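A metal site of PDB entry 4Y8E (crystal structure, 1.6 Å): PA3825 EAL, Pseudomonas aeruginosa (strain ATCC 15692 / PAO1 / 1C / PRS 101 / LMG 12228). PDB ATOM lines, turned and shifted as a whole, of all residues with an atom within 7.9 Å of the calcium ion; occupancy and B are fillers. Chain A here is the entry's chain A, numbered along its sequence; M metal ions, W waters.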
ATOM      1  N   GLU A  62      22.553  -1.593  12.722  1.00  0.00           N
ATOM      2  CA  GLU A  62      23.042  -0.226  12.950  1.00  0.00           C
ATOM      3  C   GLU A  62      24.559  -0.089  12.760  1.00  0.00           C
ATOM      4  O   GLU A  62      25.020   0.840  12.118  1.00  0.00           O
ATOM      5  CB  GLU A  62      22.659   0.222  14.365  1.00  0.00           C
ATOM      6  CG  GLU A  62      21.150   0.144  14.558  1.00  0.00           C
ATOM      7  CD  GLU A  62      20.570   1.435  15.065  1.00  0.00           C
ATOM      8  OE1 GLU A  62      20.392   1.526  16.314  1.00  0.00           O
ATOM      9  OE2 GLU A  62      20.289   2.328  14.203  1.00  0.00           O
ATOM     10  N   ILE A  67      20.936  -1.176   8.306  1.00  0.00           N
ATOM     11  CA  ILE A  67      19.591  -0.707   8.775  1.00  0.00           C
ATOM     12  C   ILE A  67      18.980   0.170   7.654  1.00  0.00           C
ATOM     13  O   ILE A  67      17.741   0.175   7.454  1.00  0.00           O
ATOM     14  CB  ILE A  67      19.629  -0.069  10.146  1.00  0.00           C
ATOM     15  CG1 ILE A  67      18.195   0.173  10.666  1.00  0.00           C
ATOM     16  CG2 ILE A  67      20.454   1.175  10.212  1.00  0.00           C
ATOM     17  CD1 ILE A  67      17.450  -1.125  10.867  1.00  0.00           C
ATOM     18  N   PHE A  97       6.970   4.978   9.607  1.00  0.00           N
ATOM     19  CA  PHE A  97       8.156   4.136   9.640  1.00  0.00           C
ATOM     20  C   PHE A  97       9.087   4.590  10.745  1.00  0.00           C
ATOM     21  O   PHE A  97       9.277   5.816  10.967  1.00  0.00           O
ATOM     22  CB  PHE A  97       8.955   4.244   8.290  1.00  0.00           C
ATOM     23  CG  PHE A  97       8.267   3.643   7.093  1.00  0.00           C
ATOM     24  CD1 PHE A  97       7.321   4.374   6.381  1.00  0.00           C
ATOM     25  CD2 PHE A  97       8.441   2.319   6.744  1.00  0.00           C
ATOM     26  CE1 PHE A  97       6.634   3.834   5.330  1.00  0.00           C
ATOM     27  CE2 PHE A  97       7.738   1.771   5.680  1.00  0.00           C
ATOM     28  CZ  PHE A  97       6.863   2.505   4.983  1.00  0.00           C
ATOM     29  N   ASN A  98       9.772   3.598  11.334  1.00  0.00           N
ATOM     30  CA  ASN A  98      10.807   3.865  12.313  1.00  0.00           C
ATOM     31  C   ASN A  98      12.126   4.053  11.516  1.00  0.00           C
ATOM     32  O   ASN A  98      12.600   3.065  10.886  1.00  0.00           O
ATOM     33  CB  ASN A  98      10.934   2.669  13.183  1.00  0.00           C
ATOM     34  CG  ASN A  98      11.991   2.844  14.282  1.00  0.00           C
ATOM     35  OD1 ASN A  98      12.993   3.532  14.123  1.00  0.00           O
ATOM     36  ND2 ASN A  98      11.784   2.149  15.422  1.00  0.00           N
ATOM     37  N   ILE A  99      12.623   5.284  11.529  1.00  0.00           N
ATOM     38  CA  ILE A  99      13.834   5.639  10.722  1.00  0.00           C
ATOM     39  C   ILE A  99      15.007   5.629  11.687  1.00  0.00           C
ATOM     40  O   ILE A  99      14.915   5.972  12.838  1.00  0.00           O
ATOM     41  CB  ILE A  99      13.622   6.969  10.094  1.00  0.00           C
ATOM     42  CG1 ILE A  99      12.410   6.928   9.122  1.00  0.00           C
ATOM     43  CG2 ILE A  99      14.862   7.491   9.288  1.00  0.00           C
ATOM     44  CD1 ILE A  99      12.380   5.833   8.107  1.00  0.00           C
ATOM     45  N   SER A 100      16.188   5.342  11.129  1.00  0.00           N
ATOM     46  CA  SER A 100      17.441   5.319  11.852  1.00  0.00           C
ATOM     47  C   SER A 100      18.221   6.642  11.543  1.00  0.00           C
ATOM     48  O   SER A 100      17.947   7.381  10.636  1.00  0.00           O
ATOM     49  CB  SER A 100      18.291   4.118  11.421  1.00  0.00           C
ATOM     50  OG  SER A 100      18.658   4.314  10.047  1.00  0.00           O
ATOM     51  N   ALA A 101      19.093   6.993  12.497  1.00  0.00           N
ATOM     52  CA  ALA A 101      19.950   8.201  12.395  1.00  0.00           C
ATOM     53  C   ALA A 101      20.778   8.149  11.132  1.00  0.00           C
ATOM     54  O   ALA A 101      20.899   9.174  10.438  1.00  0.00           O
ATOM     55  CB  ALA A 101      20.795   8.322  13.664  1.00  0.00           C
ATOM     56  N   GLU A 130       9.532   8.460  11.838  1.00  0.00           N
ATOM     57  CA  GLU A 130       9.639   8.536  13.283  1.00  0.00           C
ATOM     58  C   GLU A 130      11.102   8.363  13.739  1.00  0.00           C
ATOM     59  O   GLU A 130      11.690   7.326  13.439  1.00  0.00           O
ATOM     60  CB  GLU A 130       8.708   7.405  13.879  1.00  0.00           C
ATOM     61  CG  GLU A 130       7.287   7.535  13.296  1.00  0.00           C
ATOM     62  CD  GLU A 130       6.208   6.679  13.941  1.00  0.00           C
ATOM     63  OE1 GLU A 130       6.523   5.716  14.619  1.00  0.00           O
ATOM     64  OE2 GLU A 130       5.004   7.049  13.690  1.00  0.00           O
ATOM     65  N   LEU A 131      11.600   9.357  14.449  1.00  0.00           N
ATOM     66  CA  LEU A 131      12.912   9.371  15.014  1.00  0.00           C
ATOM     67  C   LEU A 131      12.880   9.653  16.490  1.00  0.00           C
ATOM     68  O   LEU A 131      12.205  10.557  16.918  1.00  0.00           O
ATOM     69  CB  LEU A 131      13.695  10.486  14.273  1.00  0.00           C
ATOM     70  CG  LEU A 131      14.039  10.226  12.766  1.00  0.00           C
ATOM     71  CD1 LEU A 131      14.196  11.576  12.010  1.00  0.00           C
ATOM     72  CD2 LEU A 131      15.243   9.353  12.689  1.00  0.00           C
ATOM     73  N   THR A 132      13.681   8.940  17.236  1.00  0.00           N
ATOM     74  CA  THR A 132      13.849   9.248  18.656  1.00  0.00           C
ATOM     75  C   THR A 132      14.584  10.510  18.950  1.00  0.00           C
ATOM     76  O   THR A 132      15.271  11.088  18.085  1.00  0.00           O
ATOM     77  CB  THR A 132      14.494   8.083  19.380  1.00  0.00           C
ATOM     78  OG1 THR A 132      15.878   7.991  18.945  1.00  0.00           O
ATOM     79  CG2 THR A 132      13.834   6.772  19.183  1.00  0.00           C
ATOM     80  N   GLU A 135      18.157   9.989  18.237  1.00  0.00           N
ATOM     81  CA  GLU A 135      18.457   9.982  16.799  1.00  0.00           C
ATOM     82  C   GLU A 135      18.452  11.387  16.252  1.00  0.00           C
ATOM     83  O   GLU A 135      19.296  11.741  15.403  1.00  0.00           O
ATOM     84  CB  GLU A 135      17.476   9.013  16.087  1.00  0.00           C
ATOM     85  CG  GLU A 135      17.651   7.589  16.406  1.00  0.00           C
ATOM     86  CD  GLU A 135      16.572   6.651  15.903  1.00  0.00           C
ATOM     87  OE1 GLU A 135      15.418   7.184  15.756  1.00  0.00           O
ATOM     88  OE2 GLU A 135      16.874   5.460  15.572  1.00  0.00           O
ATOM     89  N   ASP A 160       9.766   9.848  18.163  1.00  0.00           N
ATOM     90  CA  ASP A 160       9.437   8.513  18.621  1.00  0.00           C
ATOM     91  C   ASP A 160       9.834   8.297  20.054  1.00  0.00           C
ATOM     92  O   ASP A 160      10.798   8.896  20.589  1.00  0.00           O
ATOM     93  CB  ASP A 160      10.176   7.578  17.695  1.00  0.00           C
ATOM     94  CG  ASP A 160       9.754   6.163  17.779  1.00  0.00           C
ATOM     95  OD1 ASP A 160       8.708   5.797  18.494  1.00  0.00           O
ATOM     96  OD2 ASP A 160      10.367   5.272  17.136  1.00  0.00           O
ATOM     97  N   ASP A 161       9.018   7.558  20.799  1.00  0.00           N
ATOM     98  CA  ASP A 161       9.284   7.329  22.228  1.00  0.00           C
ATOM     99  C   ASP A 161       9.591   8.587  23.061  1.00  0.00           C
ATOM    100  O   ASP A 161      10.540   8.608  23.882  1.00  0.00           O
ATOM    101  CB  ASP A 161      10.377   6.294  22.413  1.00  0.00           C
ATOM    102  CG  ASP A 161      10.072   5.017  21.692  1.00  0.00           C
ATOM    103  OD1 ASP A 161       8.888   4.712  21.285  1.00  0.00           O
ATOM    104  OD2 ASP A 161      11.076   4.274  21.447  1.00  0.00           O
HETATM  105 CA    CA M   1      14.608   4.887  14.993  1.00  0.00          CA
HETATM  106  O   HOH W   1      15.944   3.099  13.920  1.00  0.00           O
HETATM  107  O   HOH W   2      12.628   5.917  15.702  1.00  0.00           O
HETATM  108  O   HOH W   3      14.492   3.791  17.196  1.00  0.00           O
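The calcium ion is bound by OD1 of Asn 98 (2.3 Å). The calcium ion is bound by water W2 (2.3 Å). The side-chain carboxylate (OE2) of Glu 135 binds the calcium ion (2.4 Å). The calcium ion is bound by O of Ile 99 (2.4 Å). Water W3 binds the calcium ion. Water W1 binds the calcium ion, 2.5 Å away. The calcium ion is bound by OE1 of Glu 135 (2.6 Å). The calcium ion has seven donor atoms within binding distance.
Water W2 bridges the side-chain carboxylate (OD2) of Asp 160 (2.8 Å) and the backbone carbonyl oxygen (O) of Glu 130 (2.8 Å).
Three residues have an atom within 4 Å of the calcium ion: Asn 98, Ile 99 and Glu 135.
The backbone NH (N) of Glu 135 sits at hydrogen-bond distance from the side-chain hydroxyl (OG1) of Thr 132. The backbone NH (N) of Ile 99 sits at hydrogen-bond distance from the backbone carbonyl oxygen (O) of Glu 130.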
